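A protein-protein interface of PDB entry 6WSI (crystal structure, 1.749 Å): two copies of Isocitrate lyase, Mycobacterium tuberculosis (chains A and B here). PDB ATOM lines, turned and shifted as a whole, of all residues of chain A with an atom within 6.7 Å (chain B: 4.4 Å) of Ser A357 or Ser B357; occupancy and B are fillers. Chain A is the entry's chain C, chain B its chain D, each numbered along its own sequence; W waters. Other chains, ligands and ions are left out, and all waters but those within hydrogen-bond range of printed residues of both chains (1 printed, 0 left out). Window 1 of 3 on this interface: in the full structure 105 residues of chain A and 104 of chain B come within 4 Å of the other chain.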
ATOM      1  N   MET A  76      -9.871  -2.804  -3.534  1.00  0.00           N
ATOM      2  CA  MET A  76      -9.956  -3.127  -2.109  1.00  0.00           C
ATOM      3  C   MET A  76      -9.984  -1.867  -1.264  1.00  0.00           C
ATOM      4  O   MET A  76     -10.804  -1.735  -0.344  1.00  0.00           O
ATOM      5  CB  MET A  76      -8.779  -3.987  -1.673  1.00  0.00           C
ATOM      6  CG  MET A  76      -8.958  -5.437  -1.866  1.00  0.00           C
ATOM      7  SD  MET A  76      -7.732  -6.387  -0.931  1.00  0.00           S
ATOM      8  CE  MET A  76      -8.101  -7.975  -1.651  1.00  0.00           C
ATOM      9  N   GLN A  79     -13.301   0.070  -1.461  1.00  0.00           N
ATOM     10  CA  GLN A  79     -14.390  -0.468  -0.644  1.00  0.00           C
ATOM     11  C   GLN A  79     -14.171  -0.163   0.836  1.00  0.00           C
ATOM     12  O   GLN A  79     -15.135   0.097   1.571  1.00  0.00           O
ATOM     13  CB  GLN A  79     -14.545  -1.974  -0.853  1.00  0.00           C
ATOM     14  CG  GLN A  79     -15.015  -2.378  -2.250  1.00  0.00           C
ATOM     15  CD  GLN A  79     -16.276  -1.657  -2.692  1.00  0.00           C
ATOM     16  OE1 GLN A  79     -17.140  -1.315  -1.874  1.00  0.00           O
ATOM     17  NE2 GLN A  79     -16.399  -1.433  -4.000  1.00  0.00           N
ATOM     18  N   GLY A 350      -7.011  -8.334   3.523  1.00  0.00           N
ATOM     19  CA  GLY A 350      -7.248  -8.463   2.093  1.00  0.00           C
ATOM     20  C   GLY A 350      -6.987  -9.869   1.563  1.00  0.00           C
ATOM     21  O   GLY A 350      -7.766 -10.394   0.765  1.00  0.00           O
ATOM     22  N   HIS A 352      -7.216 -12.680   3.159  1.00  0.00           N
ATOM     23  CA  HIS A 352      -8.211 -13.642   3.612  1.00  0.00           C
ATOM     24  C   HIS A 352      -9.577 -13.373   2.993  1.00  0.00           C
ATOM     25  O   HIS A 352     -10.288 -14.318   2.645  1.00  0.00           O
ATOM     26  CB  HIS A 352      -8.274 -13.649   5.138  1.00  0.00           C
ATOM     27  CG  HIS A 352      -7.158 -14.427   5.754  1.00  0.00           C
ATOM     28  ND1 HIS A 352      -7.109 -15.803   5.706  1.00  0.00           N
ATOM     29  CD2 HIS A 352      -6.020 -14.030   6.372  1.00  0.00           C
ATOM     30  CE1 HIS A 352      -6.005 -16.222   6.300  1.00  0.00           C
ATOM     31  NE2 HIS A 352      -5.328 -15.165   6.713  1.00  0.00           N
ATOM     32  N   ALA A 353      -9.955 -12.105   2.828  1.00  0.00           N
ATOM     33  CA  ALA A 353     -11.215 -11.804   2.154  1.00  0.00           C
ATOM     34  C   ALA A 353     -11.193 -12.310   0.716  1.00  0.00           C
ATOM     35  O   ALA A 353     -12.147 -12.950   0.257  1.00  0.00           O
ATOM     36  CB  ALA A 353     -11.484 -10.298   2.194  1.00  0.00           C
ATOM     37  N   LEU A 354     -10.091 -12.044  -0.003  1.00  0.00           N
ATOM     38  CA  LEU A 354      -9.987 -12.435  -1.408  1.00  0.00           C
ATOM     39  C   LEU A 354      -9.979 -13.954  -1.556  1.00  0.00           C
ATOM     40  O   LEU A 354     -10.701 -14.515  -2.393  1.00  0.00           O
ATOM     41  CB  LEU A 354      -8.722 -11.822  -2.026  1.00  0.00           C
ATOM     42  CG  LEU A 354      -8.432 -12.047  -3.525  1.00  0.00           C
ATOM     43  CD1 LEU A 354      -7.578 -10.891  -4.076  1.00  0.00           C
ATOM     44  CD2 LEU A 354      -7.751 -13.394  -3.822  1.00  0.00           C
ATOM     45  N   ASN A 355      -9.151 -14.638  -0.765  1.00  0.00           N
ATOM     46  CA  ASN A 355      -9.011 -16.079  -0.930  1.00  0.00           C
ATOM     47  C   ASN A 355     -10.276 -16.814  -0.495  1.00  0.00           C
ATOM     48  O   ASN A 355     -10.721 -17.750  -1.174  1.00  0.00           O
ATOM     49  CB  ASN A 355      -7.797 -16.580  -0.155  1.00  0.00           C
ATOM     50  CG  ASN A 355      -6.504 -16.432  -0.944  1.00  0.00           C
ATOM     51  OD1 ASN A 355      -6.115 -17.334  -1.692  1.00  0.00           O
ATOM     52  ND2 ASN A 355      -5.842 -15.279  -0.792  1.00  0.00           N
ATOM     53  N   TYR A 356     -10.882 -16.397   0.617  1.00  0.00           N
ATOM     54  CA  TYR A 356     -12.076 -17.097   1.074  1.00  0.00           C
ATOM     55  C   TYR A 356     -13.246 -16.848   0.130  1.00  0.00           C
ATOM     56  O   TYR A 356     -13.969 -17.786  -0.224  1.00  0.00           O
ATOM     57  CB  TYR A 356     -12.456 -16.688   2.505  1.00  0.00           C
ATOM     58  CG  TYR A 356     -13.781 -17.326   2.879  1.00  0.00           C
ATOM     59  CD1 TYR A 356     -13.853 -18.685   3.156  1.00  0.00           C
ATOM     60  CD2 TYR A 356     -14.963 -16.590   2.873  1.00  0.00           C
ATOM     61  CE1 TYR A 356     -15.068 -19.298   3.449  1.00  0.00           C
ATOM     62  CE2 TYR A 356     -16.179 -17.193   3.162  1.00  0.00           C
ATOM     63  CZ  TYR A 356     -16.219 -18.545   3.452  1.00  0.00           C
ATOM     64  OH  TYR A 356     -17.422 -19.153   3.735  1.00  0.00           O
ATOM     65  N   SER A 357     -13.439 -15.600  -0.307  1.00  0.00           N
ATOM     66  CA  SER A 357     -14.605 -15.299  -1.137  1.00  0.00           C
ATOM     67  C   SER A 357     -14.532 -16.001  -2.492  1.00  0.00           C
ATOM     68  O   SER A 357     -15.563 -16.431  -3.019  1.00  0.00           O
ATOM     69  CB  SER A 357     -14.771 -13.790  -1.314  1.00  0.00           C
ATOM     70  OG  SER A 357     -13.764 -13.217  -2.139  1.00  0.00           O
ATOM     71  N   MET A 358     -13.334 -16.142  -3.071  1.00  0.00           N
ATOM     72  CA  MET A 358     -13.269 -16.854  -4.351  1.00  0.00           C
ATOM     73  C   MET A 358     -13.381 -18.363  -4.160  1.00  0.00           C
ATOM     74  O   MET A 358     -13.963 -19.052  -5.005  1.00  0.00           O
ATOM     75  CB  MET A 358     -11.979 -16.515  -5.105  1.00  0.00           C
ATOM     76  CG  MET A 358     -11.900 -17.135  -6.529  1.00  0.00           C
ATOM     77  SD  MET A 358     -13.367 -16.786  -7.534  1.00  0.00           S
ATOM     78  CE  MET A 358     -13.141 -15.063  -7.920  1.00  0.00           C
ATOM     79  N   PHE A 359     -12.825 -18.907  -3.076  1.00  0.00           N
ATOM     80  CA  PHE A 359     -13.025 -20.334  -2.847  1.00  0.00           C
ATOM     81  C   PHE A 359     -14.501 -20.644  -2.664  1.00  0.00           C
ATOM     82  O   PHE A 359     -15.011 -21.622  -3.220  1.00  0.00           O
ATOM     83  CB  PHE A 359     -12.244 -20.835  -1.631  1.00  0.00           C
ATOM     84  CG  PHE A 359     -12.503 -22.295  -1.330  1.00  0.00           C
ATOM     85  CD1 PHE A 359     -11.749 -23.284  -1.941  1.00  0.00           C
ATOM     86  CD2 PHE A 359     -13.543 -22.676  -0.482  1.00  0.00           C
ATOM     87  CE1 PHE A 359     -12.011 -24.628  -1.699  1.00  0.00           C
ATOM     88  CE2 PHE A 359     -13.809 -24.010  -0.236  1.00  0.00           C
ATOM     89  CZ  PHE A 359     -13.043 -24.988  -0.838  1.00  0.00           C
ATOM     90  N   ASP A 360     -15.199 -19.820  -1.885  1.00  0.00           N
ATOM     91  CA  ASP A 360     -16.616 -20.053  -1.625  1.00  0.00           C
ATOM     92  C   ASP A 360     -17.425 -19.974  -2.913  1.00  0.00           C
ATOM     93  O   ASP A 360     -18.273 -20.836  -3.181  1.00  0.00           O
ATOM     94  CB  ASP A 360     -17.130 -19.040  -0.602  1.00  0.00           C
ATOM     95  CG  ASP A 360     -18.550 -19.343  -0.138  1.00  0.00           C
ATOM     96  OD1 ASP A 360     -18.770 -20.430   0.424  1.00  0.00           O
ATOM     97  OD2 ASP A 360     -19.440 -18.494  -0.339  1.00  0.00           O
ATOM     98  N   LEU A 361     -17.175 -18.945  -3.723  1.00  0.00           N
ATOM     99  CA  LEU A 361     -17.879 -18.814  -4.994  1.00  0.00           C
ATOM    100  C   LEU A 361     -17.554 -19.980  -5.922  1.00  0.00           C
ATOM    101  O   LEU A 361     -18.459 -20.602  -6.498  1.00  0.00           O
ATOM    102  CB  LEU A 361     -17.545 -17.474  -5.656  1.00  0.00           C
ATOM    103  CG  LEU A 361     -18.155 -17.284  -7.052  1.00  0.00           C
ATOM    104  CD1 LEU A 361     -19.682 -17.268  -6.966  1.00  0.00           C
ATOM    105  CD2 LEU A 361     -17.650 -16.020  -7.746  1.00  0.00           C
ATOM    106  N   ALA A 362     -16.264 -20.307  -6.074  1.00  0.00           N
ATOM    107  CA  ALA A 362     -15.896 -21.321  -7.053  1.00  0.00           C
ATOM    108  C   ALA A 362     -16.348 -22.709  -6.621  1.00  0.00           C
ATOM    109  O   ALA A 362     -16.679 -23.543  -7.477  1.00  0.00           O
ATOM    110  CB  ALA A 362     -14.386 -21.299  -7.297  1.00  0.00           C
ATOM    111  N   LEU A 376     -24.464 -14.681  -4.878  1.00  0.00           N
ATOM    112  CA  LEU A 376     -23.596 -13.528  -4.655  1.00  0.00           C
ATOM    113  C   LEU A 376     -24.239 -12.251  -5.178  1.00  0.00           C
ATOM    114  O   LEU A 376     -24.248 -11.225  -4.486  1.00  0.00           O
ATOM    115  CB  LEU A 376     -22.227 -13.754  -5.312  1.00  0.00           C
ATOM    116  CG  LEU A 376     -21.250 -12.571  -5.324  1.00  0.00           C
ATOM    117  CD1 LEU A 376     -21.014 -12.022  -3.912  1.00  0.00           C
ATOM    118  CD2 LEU A 376     -19.916 -12.960  -5.987  1.00  0.00           C
ATOM    119  N   ARG A 379     -26.776 -11.017  -2.808  1.00  0.00           N
ATOM    120  CA  ARG A 379     -26.162 -10.397  -1.632  1.00  0.00           C
ATOM    121  C   ARG A 379     -25.628  -9.004  -1.952  1.00  0.00           C
ATOM    122  O   ARG A 379     -25.670  -8.104  -1.104  1.00  0.00           O
ATOM    123  CB  ARG A 379     -25.036 -11.270  -1.083  1.00  0.00           C
ATOM    124  CG  ARG A 379     -25.484 -12.587  -0.497  1.00  0.00           C
ATOM    125  CD  ARG A 379     -24.470 -13.154   0.482  1.00  0.00           C
ATOM    126  NE  ARG A 379     -23.169 -13.395  -0.131  1.00  0.00           N
ATOM    127  CZ  ARG A 379     -22.810 -14.550  -0.689  1.00  0.00           C
ATOM    128  NH1 ARG A 379     -23.668 -15.561  -0.712  1.00  0.00           N
ATOM    129  NH2 ARG A 379     -21.600 -14.699  -1.226  1.00  0.00           N
ATOM    130  N   TYR A 388     -23.255   0.071  -0.506  1.00  0.00           N
ATOM    131  CA  TYR A 388     -22.468  -0.599  -1.539  1.00  0.00           C
ATOM    132  C   TYR A 388     -22.902  -0.153  -2.928  1.00  0.00           C
ATOM    133  O   TYR A 388     -24.098  -0.108  -3.228  1.00  0.00           O
ATOM    134  CB  TYR A 388     -22.633  -2.109  -1.398  1.00  0.00           C
ATOM    135  CG  TYR A 388     -21.819  -2.987  -2.326  1.00  0.00           C
ATOM    136  CD1 TYR A 388     -20.438  -3.101  -2.191  1.00  0.00           C
ATOM    137  CD2 TYR A 388     -22.445  -3.753  -3.301  1.00  0.00           C
ATOM    138  CE1 TYR A 388     -19.700  -3.946  -3.023  1.00  0.00           C
ATOM    139  CE2 TYR A 388     -21.712  -4.606  -4.134  1.00  0.00           C
ATOM    140  CZ  TYR A 388     -20.348  -4.697  -3.985  1.00  0.00           C
ATOM    141  OH  TYR A 388     -19.644  -5.533  -4.819  1.00  0.00           O
ATOM    142  N   ALA B 353     -16.596 -10.750  -6.456  1.00  0.00           N
ATOM    143  CA  ALA B 353     -16.225 -11.408  -5.207  1.00  0.00           C
ATOM    144  C   ALA B 353     -15.267 -10.536  -4.405  1.00  0.00           C
ATOM    145  O   ALA B 353     -15.405 -10.410  -3.183  1.00  0.00           O
ATOM    146  CB  ALA B 353     -15.600 -12.778  -5.474  1.00  0.00           C
ATOM    147  N   LEU B 354     -14.313  -9.895  -5.088  1.00  0.00           N
ATOM    148  CA  LEU B 354     -13.343  -9.037  -4.402  1.00  0.00           C
ATOM    149  C   LEU B 354     -14.009  -7.804  -3.803  1.00  0.00           C
ATOM    150  O   LEU B 354     -13.785  -7.474  -2.632  1.00  0.00           O
ATOM    151  CB  LEU B 354     -12.227  -8.616  -5.369  1.00  0.00           C
ATOM    152  CG  LEU B 354     -11.081  -7.737  -4.826  1.00  0.00           C
ATOM    153  CD1 LEU B 354      -9.818  -7.962  -5.654  1.00  0.00           C
ATOM    154  CD2 LEU B 354     -11.429  -6.242  -4.786  1.00  0.00           C
ATOM    155  N   ASN B 355     -14.788  -7.076  -4.604  1.00  0.00           N
ATOM    156  CA  ASN B 355     -15.384  -5.835  -4.113  1.00  0.00           C
ATOM    157  C   ASN B 355     -16.415  -6.102  -3.025  1.00  0.00           C
ATOM    158  O   ASN B 355     -16.450  -5.396  -2.003  1.00  0.00           O
ATOM    159  CB  ASN B 355     -16.013  -5.054  -5.264  1.00  0.00           C
ATOM    160  CG  ASN B 355     -14.995  -4.218  -6.014  1.00  0.00           C
ATOM    161  OD1 ASN B 355     -14.772  -3.053  -5.683  1.00  0.00           O
ATOM    162  ND2 ASN B 355     -14.347  -4.823  -7.013  1.00  0.00           N
ATOM    163  N   TYR B 356     -17.261  -7.119  -3.208  1.00  0.00           N
ATOM    164  CA  TYR B 356     -18.268  -7.386  -2.184  1.00  0.00           C
ATOM    165  C   TYR B 356     -17.630  -7.860  -0.884  1.00  0.00           C
ATOM    166  O   TYR B 356     -18.026  -7.410   0.202  1.00  0.00           O
ATOM    167  CB  TYR B 356     -19.290  -8.426  -2.655  1.00  0.00           C
ATOM    168  CG  TYR B 356     -20.219  -8.779  -1.520  1.00  0.00           C
ATOM    169  CD1 TYR B 356     -21.187  -7.873  -1.094  1.00  0.00           C
ATOM    170  CD2 TYR B 356     -20.091  -9.980  -0.828  1.00  0.00           C
ATOM    171  CE1 TYR B 356     -22.024  -8.164  -0.027  1.00  0.00           C
ATOM    172  CE2 TYR B 356     -20.927 -10.279   0.240  1.00  0.00           C
ATOM    173  CZ  TYR B 356     -21.889  -9.362   0.632  1.00  0.00           C
ATOM    174  OH  TYR B 356     -22.721  -9.655   1.685  1.00  0.00           O
ATOM    175  N   SER B 357     -16.648  -8.773  -0.964  1.00  0.00           N
ATOM    176  CA  SER B 357     -16.117  -9.353   0.267  1.00  0.00           C
ATOM    177  C   SER B 357     -15.384  -8.304   1.100  1.00  0.00           C
ATOM    178  O   SER B 357     -15.498  -8.303   2.331  1.00  0.00           O
ATOM    179  CB  SER B 357     -15.216 -10.559  -0.022  1.00  0.00           C
ATOM    180  OG  SER B 357     -14.046 -10.214  -0.744  1.00  0.00           O
ATOM    181  N   MET B 358     -14.663  -7.383   0.453  1.00  0.00           N
ATOM    182  CA  MET B 358     -13.976  -6.347   1.221  1.00  0.00           C
ATOM    183  C   MET B 358     -14.960  -5.312   1.746  1.00  0.00           C
ATOM    184  O   MET B 358     -14.785  -4.796   2.854  1.00  0.00           O
ATOM    185  CB  MET B 358     -12.870  -5.678   0.391  1.00  0.00           C
ATOM    186  CG  MET B 358     -12.005  -4.666   1.194  1.00  0.00           C
ATOM    187  SD  MET B 358     -11.426  -5.288   2.795  1.00  0.00           S
ATOM    188  CE  MET B 358     -10.249  -6.527   2.273  1.00  0.00           C
ATOM    189  N   PHE B 359     -15.998  -4.980   0.974  1.00  0.00           N
ATOM    190  CA  PHE B 359     -16.994  -4.056   1.524  1.00  0.00           C
ATOM    191  C   PHE B 359     -17.667  -4.658   2.747  1.00  0.00           C
ATOM    192  O   PHE B 359     -17.864  -3.975   3.764  1.00  0.00           O
ATOM    193  CB  PHE B 359     -18.051  -3.673   0.490  1.00  0.00           C
ATOM    194  CG  PHE B 359     -19.159  -2.817   1.069  1.00  0.00           C
ATOM    195  CD1 PHE B 359     -19.000  -1.445   1.195  1.00  0.00           C
ATOM    196  CD2 PHE B 359     -20.331  -3.395   1.536  1.00  0.00           C
ATOM    197  CE1 PHE B 359     -20.006  -0.657   1.746  1.00  0.00           C
ATOM    198  CE2 PHE B 359     -21.340  -2.608   2.093  1.00  0.00           C
ATOM    199  CZ  PHE B 359     -21.176  -1.253   2.202  1.00  0.00           C
ATOM    200  N   ASP B 360     -18.020  -5.939   2.670  1.00  0.00           N
ATOM    201  CA  ASP B 360     -18.739  -6.569   3.772  1.00  0.00           C
ATOM    202  C   ASP B 360     -17.872  -6.623   5.022  1.00  0.00           C
ATOM    203  O   ASP B 360     -18.332  -6.298   6.123  1.00  0.00           O
ATOM    204  CB  ASP B 360     -19.200  -7.968   3.365  1.00  0.00           C
ATOM    205  CG  ASP B 360     -20.066  -8.634   4.433  1.00  0.00           C
ATOM    206  OD1 ASP B 360     -21.133  -8.088   4.755  1.00  0.00           O
ATOM    207  OD2 ASP B 360     -19.668  -9.695   4.949  1.00  0.00           O
ATOM    208  N   LEU B 361     -16.611  -7.031   4.867  1.00  0.00           N
ATOM    209  CA  LEU B 361     -15.688  -7.045   5.995  1.00  0.00           C
ATOM    210  C   LEU B 361     -15.470  -5.638   6.546  1.00  0.00           C
ATOM    211  O   LEU B 361     -15.544  -5.413   7.760  1.00  0.00           O
ATOM    212  CB  LEU B 361     -14.353  -7.664   5.572  1.00  0.00           C
ATOM    213  CG  LEU B 361     -13.259  -7.676   6.649  1.00  0.00           C
ATOM    214  CD1 LEU B 361     -13.739  -8.475   7.853  1.00  0.00           C
ATOM    215  CD2 LEU B 361     -11.942  -8.257   6.102  1.00  0.00           C
HETATM  216  O   HOH W   1     -25.417  -8.367   1.680  1.00  0.00           O
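Among the printed residues, merely in contact across the chains: Gln A79 with Phe B359 (3.5 Å), Tyr A388 with Phe B359 (3.5 Å), Met A76 with Met B358 (3.5 Å), Gly A350 with Met B358 (3.6 Å), Tyr A388 with Asn B355 (3.7 Å), Arg A379 with Tyr B356 (3.8 Å), Leu A376 with Tyr B356 (3.8 Å), Met A76 with Leu B354 (3.9 Å) and Ala A353 with Met B358 (3.97 Å).
OG of Ser A357 sits at hydrogen-bond distance from O of Ala A353 (2.9 Å).
O of Leu A354 sits at hydrogen-bond distance from OG of Ser A357 (3.3 Å).
The backbone carbonyl oxygen (O) of Ala B353 sits at hydrogen-bond distance from the side-chain hydroxyl (OG) of Ser B357, 2.8 Å away.
O of Leu B354 lies within hydrogen-bond range of OG of Ser B357, 3.3 Å away.
Ala A353 touches Ser B357, and with the chains exchanged Ser A357 touches Ala B353.
Ala A353 touches Met B358, but with the chains exchanged Met A358 does not touch Ala B353 (4.2 Å).
Ser A357 touches its own counterpart, Ser B357.
Of the 14 pairs that touch across the chains among the printed residues, 3 have their exchanged pair printed and touching as well.
Ser A357 touches just these residues of chain B: Ala B353 and Ser B357.
Of chain A, only Ala A353 (3.5 Å) and Ser A357 (3.3 Å) come within 4 Å of Ser B357.
Printed residues of chain A within 4 Å of Tyr B356: Leu A376 (3.8 Å), Arg A379 (3.8 Å) and Tyr A388 (3.3 Å).
Of the printed residues of chain B, Arg A379 touches Tyr B356 (3.8 Å).
Leu A354 touches none of the printed residues of chain B.
Asn A355 touches none of the printed residues of chain B.
The nearest printed residue of chain B that does not touch Ser A357 is Leu B354 (4.5 Å).
The nearest residue of chain A that does not touch Ser B357 is Leu A354 (4.4 Å).
The nearest printed residue of chain A that does not touch Leu B354 is Leu A354 (4.01 Å).
NE2 of Gln A79 is in hydrogen-bond range of OD1 of Asn B355 (2.8 Å).
The backbone carbonyl oxygen (O) of Ala A353 sits at hydrogen-bond distance from the side-chain hydroxyl (OG) of Ser B357 (3.5 Å).
The side-chain hydroxyl of Ser A357 is in hydrogen-bond range of the backbone carbonyl oxygen of Ala B353, 3.4 Å away.
The side-chain hydroxyl (OG) of Ser B357 is in hydrogen-bond range of the side-chain hydroxyl (OG) of Ser A357, 3.3 Å away.
The backbone NH of Tyr B356 is in hydrogen-bond range of the side-chain hydroxyl of Tyr A388 (3.3 Å).
Water W1 bridges the backbone carbonyl oxygen of Arg A379 and the side-chain hydroxyl of Tyr B356.
Printed residues of chain B that touch a printed residue of chain A: Ala B353, Leu B354, Asn B355, Tyr B356, Ser B357, Met B358 and Phe B359.
Hydrophobic or aromatic side chains of chain B within 4 Å of the printed part of chain A: Ala B353, Leu B354, Tyr B356, Met B358 and Phe B359.
Hydrophobic or aromatic side chains of chain A that line the printed part of chain B: Met A76, Ala A353, Leu A376 and Tyr A388.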
